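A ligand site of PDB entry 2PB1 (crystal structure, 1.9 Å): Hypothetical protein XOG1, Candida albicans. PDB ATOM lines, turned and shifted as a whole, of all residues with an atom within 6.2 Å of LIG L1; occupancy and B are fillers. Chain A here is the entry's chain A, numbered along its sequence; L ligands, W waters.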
ATOM      1  N   GLU A  27     -24.631  -1.095  26.932  1.00  0.00           N
ATOM      2  CA  GLU A  27     -23.788  -2.104  26.308  1.00  0.00           C
ATOM      3  C   GLU A  27     -22.406  -2.076  26.924  1.00  0.00           C
ATOM      4  O   GLU A  27     -21.732  -1.053  26.865  1.00  0.00           O
ATOM      5  CB  GLU A  27     -23.719  -1.919  24.792  1.00  0.00           C
ATOM      6  CG  GLU A  27     -25.095  -1.920  24.146  1.00  0.00           C
ATOM      7  CD  GLU A  27     -25.024  -1.959  22.623  1.00  0.00           C
ATOM      8  OE1 GLU A  27     -24.094  -2.612  22.106  1.00  0.00           O
ATOM      9  OE2 GLU A  27     -25.890  -1.305  21.980  1.00  0.00           O
ATOM     10  N   TYR A  29     -19.356  -3.027  26.175  1.00  0.00           N
ATOM     11  CA  TYR A  29     -18.193  -2.585  25.408  1.00  0.00           C
ATOM     12  C   TYR A  29     -18.194  -1.059  25.153  1.00  0.00           C
ATOM     13  O   TYR A  29     -17.108  -0.461  24.973  1.00  0.00           O
ATOM     14  CB  TYR A  29     -18.010  -3.384  24.119  1.00  0.00           C
ATOM     15  CG  TYR A  29     -18.800  -2.875  22.928  1.00  0.00           C
ATOM     16  CD1 TYR A  29     -20.089  -3.316  22.682  1.00  0.00           C
ATOM     17  CD2 TYR A  29     -18.243  -1.964  22.028  1.00  0.00           C
ATOM     18  CE1 TYR A  29     -20.810  -2.841  21.546  1.00  0.00           C
ATOM     19  CE2 TYR A  29     -18.926  -1.515  20.909  1.00  0.00           C
ATOM     20  CZ  TYR A  29     -20.227  -1.952  20.674  1.00  0.00           C
ATOM     21  OH  TYR A  29     -20.911  -1.481  19.555  1.00  0.00           O
ATOM     22  N   MET A  30     -19.367  -0.438  25.221  1.00  0.00           N
ATOM     23  CA  MET A  30     -19.518   0.978  24.931  1.00  0.00           C
ATOM     24  C   MET A  30     -19.310   1.845  26.174  1.00  0.00           C
ATOM     25  O   MET A  30     -18.755   2.933  26.055  1.00  0.00           O
ATOM     26  CB  MET A  30     -20.879   1.265  24.339  1.00  0.00           C
ATOM     27  CG  MET A  30     -21.085   0.571  22.993  1.00  0.00           C
ATOM     28  SD  MET A  30     -22.670   0.973  22.219  1.00  0.00           S
ATOM     29  CE  MET A  30     -22.356   2.669  21.701  1.00  0.00           C
ATOM     30  N   ARG A  92     -30.426   7.598  14.563  1.00  0.00           N
ATOM     31  CA  ARG A  92     -31.202   6.454  15.014  1.00  0.00           C
ATOM     32  C   ARG A  92     -31.096   6.281  16.524  1.00  0.00           C
ATOM     33  O   ARG A  92     -29.982   6.263  17.064  1.00  0.00           O
ATOM     34  CB  ARG A  92     -30.676   5.194  14.323  1.00  0.00           C
ATOM     35  CG  ARG A  92     -31.467   3.957  14.596  1.00  0.00           C
ATOM     36  CD  ARG A  92     -30.867   2.923  13.673  1.00  0.00           C
ATOM     37  NE  ARG A  92     -31.405   1.620  13.754  1.00  0.00           N
ATOM     38  CZ  ARG A  92     -30.804   0.562  14.298  1.00  0.00           C
ATOM     39  NH1 ARG A  92     -29.615   0.626  14.870  1.00  0.00           N
ATOM     40  NH2 ARG A  92     -31.428  -0.578  14.253  1.00  0.00           N
ATOM     41  N   ASP A 133     -36.027   3.191  17.359  1.00  0.00           N
ATOM     42  CA  ASP A 133     -35.727   1.800  17.122  1.00  0.00           C
ATOM     43  C   ASP A 133     -35.972   1.015  18.403  1.00  0.00           C
ATOM     44  O   ASP A 133     -35.343   1.284  19.415  1.00  0.00           O
ATOM     45  CB  ASP A 133     -34.277   1.673  16.609  1.00  0.00           C
ATOM     46  CG  ASP A 133     -33.544   0.437  17.093  1.00  0.00           C
ATOM     47  OD1 ASP A 133     -34.102  -0.658  17.042  1.00  0.00           O
ATOM     48  OD2 ASP A 133     -32.382   0.561  17.486  1.00  0.00           O
ATOM     49  N   HIS A 135     -35.122  -1.727  20.397  1.00  0.00           N
ATOM     50  CA  HIS A 135     -33.870  -2.431  20.353  1.00  0.00           C
ATOM     51  C   HIS A 135     -33.897  -3.730  21.149  1.00  0.00           C
ATOM     52  O   HIS A 135     -33.091  -4.613  20.918  1.00  0.00           O
ATOM     53  CB  HIS A 135     -32.762  -1.518  20.889  1.00  0.00           C
ATOM     54  CG  HIS A 135     -31.441  -1.695  20.188  1.00  0.00           C
ATOM     55  ND1 HIS A 135     -31.201  -1.250  18.903  1.00  0.00           N
ATOM     56  CD2 HIS A 135     -30.262  -2.205  20.629  1.00  0.00           C
ATOM     57  CE1 HIS A 135     -29.952  -1.497  18.581  1.00  0.00           C
ATOM     58  NE2 HIS A 135     -29.352  -2.087  19.609  1.00  0.00           N
ATOM     59  N   PHE A 144     -28.487 -11.310  22.258  1.00  0.00           N
ATOM     60  CA  PHE A 144     -27.341 -10.430  22.329  1.00  0.00           C
ATOM     61  C   PHE A 144     -27.458  -9.586  23.592  1.00  0.00           C
ATOM     62  O   PHE A 144     -28.550  -9.227  24.028  1.00  0.00           O
ATOM     63  CB  PHE A 144     -27.273  -9.458  21.142  1.00  0.00           C
ATOM     64  CG  PHE A 144     -27.328 -10.119  19.782  1.00  0.00           C
ATOM     65  CD1 PHE A 144     -26.847 -11.417  19.577  1.00  0.00           C
ATOM     66  CD2 PHE A 144     -27.779  -9.394  18.687  1.00  0.00           C
ATOM     67  CE1 PHE A 144     -26.902 -11.991  18.316  1.00  0.00           C
ATOM     68  CE2 PHE A 144     -27.791  -9.967  17.411  1.00  0.00           C
ATOM     69  CZ  PHE A 144     -27.353 -11.266  17.231  1.00  0.00           C
ATOM     70  N   ASN A 146     -27.030  -6.504  23.805  1.00  0.00           N
ATOM     71  CA  ASN A 146     -27.666  -5.243  23.401  1.00  0.00           C
ATOM     72  C   ASN A 146     -29.220  -5.284  23.254  1.00  0.00           C
ATOM     73  O   ASN A 146     -29.878  -4.244  23.067  1.00  0.00           O
ATOM     74  CB  ASN A 146     -26.971  -4.712  22.144  1.00  0.00           C
ATOM     75  CG  ASN A 146     -27.076  -5.651  20.993  1.00  0.00           C
ATOM     76  OD1 ASN A 146     -28.176  -5.875  20.475  1.00  0.00           O
ATOM     77  ND2 ASN A 146     -25.948  -6.228  20.587  1.00  0.00           N
ATOM     78  N   SER A 147     -29.816  -6.471  23.368  1.00  0.00           N
ATOM     79  CA  SER A 147     -31.276  -6.608  23.535  1.00  0.00           C
ATOM     80  C   SER A 147     -31.757  -6.383  24.972  1.00  0.00           C
ATOM     81  O   SER A 147     -32.970  -6.373  25.214  1.00  0.00           O
ATOM     82  CB  SER A 147     -31.763  -8.003  23.100  1.00  0.00           C
ATOM     83  OG  SER A 147     -31.378  -9.027  24.024  1.00  0.00           O
ATOM     84  N   ASN A 191     -35.073  -4.321  16.416  1.00  0.00           N
ATOM     85  CA  ASN A 191     -33.678  -4.434  15.998  1.00  0.00           C
ATOM     86  C   ASN A 191     -33.213  -5.891  15.938  1.00  0.00           C
ATOM     87  O   ASN A 191     -33.328  -6.612  16.934  1.00  0.00           O
ATOM     88  CB  ASN A 191     -32.762  -3.678  16.966  1.00  0.00           C
ATOM     89  CG  ASN A 191     -31.345  -3.689  16.504  1.00  0.00           C
ATOM     90  OD1 ASN A 191     -31.034  -3.114  15.462  1.00  0.00           O
ATOM     91  ND2 ASN A 191     -30.473  -4.355  17.248  1.00  0.00           N
ATOM     92  N   GLU A 192     -32.656  -6.312  14.809  1.00  0.00           N
ATOM     93  CA  GLU A 192     -31.895  -7.583  14.719  1.00  0.00           C
ATOM     94  C   GLU A 192     -32.560  -8.844  15.332  1.00  0.00           C
ATOM     95  O   GLU A 192     -31.939  -9.584  16.121  1.00  0.00           O
ATOM     96  CB  GLU A 192     -30.468  -7.395  15.267  1.00  0.00           C
ATOM     97  CG  GLU A 192     -29.612  -6.411  14.449  1.00  0.00           C
ATOM     98  CD  GLU A 192     -28.145  -6.333  14.825  1.00  0.00           C
ATOM     99  OE1 GLU A 192     -27.765  -6.835  15.903  1.00  0.00           O
ATOM    100  OE2 GLU A 192     -27.336  -5.779  14.029  1.00  0.00           O
ATOM    101  N   HIS A 253     -27.843  -4.315   8.187  1.00  0.00           N
ATOM    102  CA  HIS A 253     -26.662  -4.060   8.998  1.00  0.00           C
ATOM    103  C   HIS A 253     -25.486  -4.831   8.399  1.00  0.00           C
ATOM    104  O   HIS A 253     -25.657  -5.867   7.779  1.00  0.00           O
ATOM    105  CB  HIS A 253     -26.929  -4.512  10.426  1.00  0.00           C
ATOM    106  CG  HIS A 253     -28.025  -3.769  11.107  1.00  0.00           C
ATOM    107  ND1 HIS A 253     -28.470  -4.083  12.369  1.00  0.00           N
ATOM    108  CD2 HIS A 253     -28.794  -2.734  10.690  1.00  0.00           C
ATOM    109  CE1 HIS A 253     -29.437  -3.263  12.706  1.00  0.00           C
ATOM    110  NE2 HIS A 253     -29.646  -2.417  11.717  1.00  0.00           N
ATOM    111  N   TYR A 255     -21.262  -5.837   8.930  1.00  0.00           N
ATOM    112  CA  TYR A 255     -19.928  -5.913   9.551  1.00  0.00           C
ATOM    113  C   TYR A 255     -19.080  -7.021   8.918  1.00  0.00           C
ATOM    114  O   TYR A 255     -19.600  -7.919   8.227  1.00  0.00           O
ATOM    115  CB  TYR A 255     -20.050  -6.192  11.063  1.00  0.00           C
ATOM    116  CG  TYR A 255     -20.797  -5.139  11.859  1.00  0.00           C
ATOM    117  CD1 TYR A 255     -20.283  -3.846  12.052  1.00  0.00           C
ATOM    118  CD2 TYR A 255     -22.025  -5.451  12.439  1.00  0.00           C
ATOM    119  CE1 TYR A 255     -21.008  -2.892  12.787  1.00  0.00           C
ATOM    120  CE2 TYR A 255     -22.730  -4.532  13.192  1.00  0.00           C
ATOM    121  CZ  TYR A 255     -22.224  -3.266  13.377  1.00  0.00           C
ATOM    122  OH  TYR A 255     -22.969  -2.401  14.135  1.00  0.00           O
ATOM    123  N   PHE A 258     -17.275 -10.603  12.826  1.00  0.00           N
ATOM    124  CA  PHE A 258     -17.869 -11.545  13.770  1.00  0.00           C
ATOM    125  C   PHE A 258     -17.706 -13.025  13.397  1.00  0.00           C
ATOM    126  O   PHE A 258     -18.486 -13.878  13.844  1.00  0.00           O
ATOM    127  CB  PHE A 258     -19.310 -11.184  14.108  1.00  0.00           C
ATOM    128  CG  PHE A 258     -19.431  -9.873  14.821  1.00  0.00           C
ATOM    129  CD1 PHE A 258     -18.985  -9.741  16.114  1.00  0.00           C
ATOM    130  CD2 PHE A 258     -19.980  -8.763  14.171  1.00  0.00           C
ATOM    131  CE1 PHE A 258     -19.107  -8.520  16.799  1.00  0.00           C
ATOM    132  CE2 PHE A 258     -20.107  -7.556  14.847  1.00  0.00           C
ATOM    133  CZ  PHE A 258     -19.646  -7.427  16.158  1.00  0.00           C
ATOM    134  N   GLU A 292     -26.707   0.234  10.510  1.00  0.00           N
ATOM    135  CA  GLU A 292     -25.644  -0.159  11.423  1.00  0.00           C
ATOM    136  C   GLU A 292     -24.456  -0.705  10.649  1.00  0.00           C
ATOM    137  O   GLU A 292     -24.585  -1.623   9.812  1.00  0.00           O
ATOM    138  CB  GLU A 292     -26.169  -1.203  12.412  1.00  0.00           C
ATOM    139  CG  GLU A 292     -25.778  -0.954  13.758  1.00  0.00           C
ATOM    140  CD  GLU A 292     -26.303  -1.975  14.757  1.00  0.00           C
ATOM    141  OE1 GLU A 292     -27.533  -2.260  14.774  1.00  0.00           O
ATOM    142  OE2 GLU A 292     -25.448  -2.472  15.539  1.00  0.00           O
ATOM    143  N   LEU A 304     -16.652  -6.563  23.301  1.00  0.00           N
ATOM    144  CA  LEU A 304     -17.498  -6.520  22.072  1.00  0.00           C
ATOM    145  C   LEU A 304     -18.367  -7.805  21.882  1.00  0.00           C
ATOM    146  O   LEU A 304     -19.544  -7.746  21.497  1.00  0.00           O
ATOM    147  CB  LEU A 304     -16.604  -6.326  20.832  1.00  0.00           C
ATOM    148  CG  LEU A 304     -17.325  -6.194  19.510  1.00  0.00           C
ATOM    149  CD1 LEU A 304     -18.252  -4.971  19.496  1.00  0.00           C
ATOM    150  CD2 LEU A 304     -16.265  -6.197  18.338  1.00  0.00           C
ATOM    151  N   TRP A 363     -22.500   3.089  13.542  1.00  0.00           N
ATOM    152  CA  TRP A 363     -22.561   2.653  14.961  1.00  0.00           C
ATOM    153  C   TRP A 363     -21.171   2.819  15.593  1.00  0.00           C
ATOM    154  O   TRP A 363     -20.266   2.034  15.271  1.00  0.00           O
ATOM    155  CB  TRP A 363     -23.017   1.177  15.087  1.00  0.00           C
ATOM    156  CG  TRP A 363     -23.262   0.859  16.530  1.00  0.00           C
ATOM    157  CD1 TRP A 363     -22.309   0.599  17.471  1.00  0.00           C
ATOM    158  CD2 TRP A 363     -24.514   0.880  17.228  1.00  0.00           C
ATOM    159  NE1 TRP A 363     -22.899   0.426  18.703  1.00  0.00           N
ATOM    160  CE2 TRP A 363     -24.249   0.590  18.594  1.00  0.00           C
ATOM    161  CE3 TRP A 363     -25.842   1.076  16.825  1.00  0.00           C
ATOM    162  CZ2 TRP A 363     -25.265   0.511  19.553  1.00  0.00           C
ATOM    163  CZ3 TRP A 363     -26.842   1.005  17.762  1.00  0.00           C
ATOM    164  CH2 TRP A 363     -26.545   0.698  19.136  1.00  0.00           C
ATOM    165  N   TRP A 373     -15.450   2.086  16.896  1.00  0.00           N
ATOM    166  CA  TRP A 373     -16.894   2.181  17.077  1.00  0.00           C
ATOM    167  C   TRP A 373     -17.368   3.612  17.480  1.00  0.00           C
ATOM    168  O   TRP A 373     -18.530   3.800  17.905  1.00  0.00           O
ATOM    169  CB  TRP A 373     -17.305   1.171  18.136  1.00  0.00           C
ATOM    170  CG  TRP A 373     -16.930  -0.256  17.782  1.00  0.00           C
ATOM    171  CD1 TRP A 373     -15.777  -0.921  18.078  1.00  0.00           C
ATOM    172  CD2 TRP A 373     -17.699  -1.154  16.974  1.00  0.00           C
ATOM    173  NE1 TRP A 373     -15.802  -2.177  17.548  1.00  0.00           N
ATOM    174  CE2 TRP A 373     -16.969  -2.350  16.855  1.00  0.00           C
ATOM    175  CE3 TRP A 373     -18.948  -1.068  16.354  1.00  0.00           C
ATOM    176  CZ2 TRP A 373     -17.439  -3.435  16.152  1.00  0.00           C
ATOM    177  CZ3 TRP A 373     -19.409  -2.149  15.651  1.00  0.00           C
ATOM    178  CH2 TRP A 373     -18.660  -3.313  15.540  1.00  0.00           C
HETATM  179  C1  LIG L   1     -25.663  -3.685  16.262  1.00  0.00           C
HETATM  180  C2  LIG L   1     -26.451  -3.614  17.558  1.00  0.00           C
HETATM  181  C3  LIG L   1     -25.692  -2.783  18.590  1.00  0.00           C
HETATM  182  C4  LIG L   1     -24.264  -3.348  18.759  1.00  0.00           C
HETATM  183  C5  LIG L   1     -23.561  -3.461  17.410  1.00  0.00           C
HETATM  184  C6  LIG L   1     -22.213  -4.199  17.468  1.00  0.00           C
HETATM  185  O1  LIG L   1     -26.452  -2.717  19.804  1.00  0.00           O
HETATM  186  O2  LIG L   1     -23.467  -2.551  19.657  1.00  0.00           O
HETATM  187  O3  LIG L   1     -24.369  -4.174  16.492  1.00  0.00           O
HETATM  188  O4  LIG L   1     -22.359  -5.559  17.895  1.00  0.00           O
HETATM  189  F1  LIG L   1     -27.649  -3.019  17.358  1.00  0.00           F
HETATM  190  C1  LG2 L   2     -23.753 -10.900  15.788  1.00  0.00           C
HETATM  191  O1  LG2 L   2     -23.242 -11.753  14.791  1.00  0.00           O
HETATM  192  C2  LG2 L   2     -22.874 -10.937  17.034  1.00  0.00           C
HETATM  193  F1  LG2 L   2     -23.032 -12.151  17.650  1.00  0.00           F
HETATM  194  C3  LG2 L   2     -23.253  -9.823  17.985  1.00  0.00           C
HETATM  195  O2  LG2 L   2     -22.314  -9.723  19.072  1.00  0.00           O
HETATM  196  C4  LG2 L   2     -23.298  -8.506  17.225  1.00  0.00           C
HETATM  197  O3  LG2 L   2     -23.866  -7.521  18.105  1.00  0.00           O
HETATM  198  C5  LG2 L   2     -24.151  -8.612  15.959  1.00  0.00           C
HETATM  199  C6  LG2 L   2     -24.101  -7.399  15.052  1.00  0.00           C
HETATM  200  O4  LG2 L   2     -25.117  -7.553  14.043  1.00  0.00           O
HETATM  201  O5  LG2 L   2     -23.694  -9.656  15.130  1.00  0.00           O
HETATM  202  C7  LG2 L   2     -24.068 -12.548  14.066  1.00  0.00           C
HETATM  203  C8  LG2 L   2     -23.608 -13.809  13.732  1.00  0.00           C
HETATM  204  N1  LG2 L   2     -22.312 -14.201  14.141  1.00  0.00           N
HETATM  205  O6  LG2 L   2     -21.418 -14.345  13.308  1.00  0.00           O
HETATM  206  O7  LG2 L   2     -22.074 -14.387  15.338  1.00  0.00           O
HETATM  207  C9  LG2 L   2     -24.435 -14.649  12.988  1.00  0.00           C
HETATM  208  C10 LG2 L   2     -25.707 -14.233  12.597  1.00  0.00           C
HETATM  209  N2  LG2 L   2     -26.547 -15.069  11.854  1.00  0.00           N
HETATM  210  O8  LG2 L   2     -27.498 -14.616  11.241  1.00  0.00           O
HETATM  211  O9  LG2 L   2     -26.349 -16.283  11.845  1.00  0.00           O
HETATM  212  C11 LG2 L   2     -26.151 -12.954  12.959  1.00  0.00           C
HETATM  213  C12 LG2 L   2     -25.330 -12.105  13.683  1.00  0.00           C
HETATM  214  O   HOH W   1     -21.587  -6.228  20.335  1.00  0.00           O
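An oxygen (O3) of LG2 L2 lies within hydrogen-bond range of an oxygen (O4) of LIG L1, 2.5 Å away.
Water W1 lies within hydrogen-bond range of an oxygen (O4) of LIG L1 (2.6 Å), the backbone carbonyl oxygen (O) of Leu 304 (2.8 Å) and an oxygen (O3) of LG2 L2 (3.4 Å).
ND2 of Asn 191 lies close to F1 of LIG L1, at 3.1 Å.
Asn 146 touches LIG L1 (CB to O1, 3.1 Å).
OE2 of Glu 192 touches C1 of LIG L1, at 3.5 Å.
Phe 258 touches LIG L1 (CZ to O4, 3.7 Å).
Trp 373 touches LIG L1.
Hydrophobic or aromatic side chains that line LIG L1: Tyr 29, His 135, Tyr 255, Phe 258, Trp 363 and Trp 373.
Within 4 Å of LIG L1: Glu 27, Tyr 29, His 135, Asn 146, Asn 191, Glu 192, Tyr 255, Phe 258, Glu 292, Trp 363 and Trp 373.
The nearest printed residue that does not touch LIG L1 is Met 30 (4.4 Å).
OE2 of Glu 292 is bonded to C1 of LIG L1 (1.4 Å).
OE1 of Glu 27 lies within hydrogen-bond range of O2 of LIG L1, 2.5 Å away.
The side-chain hydroxyl (OH) of Tyr 29 is in hydrogen-bond range of an oxygen (O2) of LIG L1 (2.8 Å).
An oxygen (O1) of LIG L1 lies within hydrogen-bond range of a ring nitrogen (NE2) of His 135 (3.0 Å).
The indole nitrogen (NE1) of Trp 363 lies within hydrogen-bond range of an oxygen (O2) of LIG L1, 3.2 Å away.
The side-chain hydroxyl of Tyr 255 is in hydrogen-bond range of an oxygen (O3) of LIG L1, at 3.3 Å.
An oxygen (O3) of LG2 L2 is in hydrogen-bond range of the side-chain amide nitrogen (ND2) of Asn 146 (3.5 Å).
O4 of LG2 L2 lies within hydrogen-bond range of OE2 of Glu 192 (2.8 Å).
OH of Tyr 255 is in hydrogen-bond range of OE2 of Glu 292 (2.8 Å).
ND1 of His 253 sits close to OE1 of Glu 292, 3.2 Å away.
OE1 of Glu 292 lies within salt-bridge range of NH1 of Arg 92, 3.6 Å away.
A ring nitrogen (NE2) of His 135 sits close to the side-chain amide nitrogen (ND2) of Asn 191 (3.5 Å).
ND1 of His 135 is in hydrogen-bond range of OD2 of Asp 133, at 2.6 Å.
The side-chain amide oxygen (OD1) of Asn 191 sits at hydrogen-bond distance from the guanidinium group (NH2) of Arg 92 (2.8 Å).
The indole nitrogen of Trp 363 lies within hydrogen-bond range of the side-chain sulfur of Met 30, 3.6 Å away.
OE2 of Glu 192 lies within hydrogen-bond range of ND1 of His 253 (2.6 Å).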
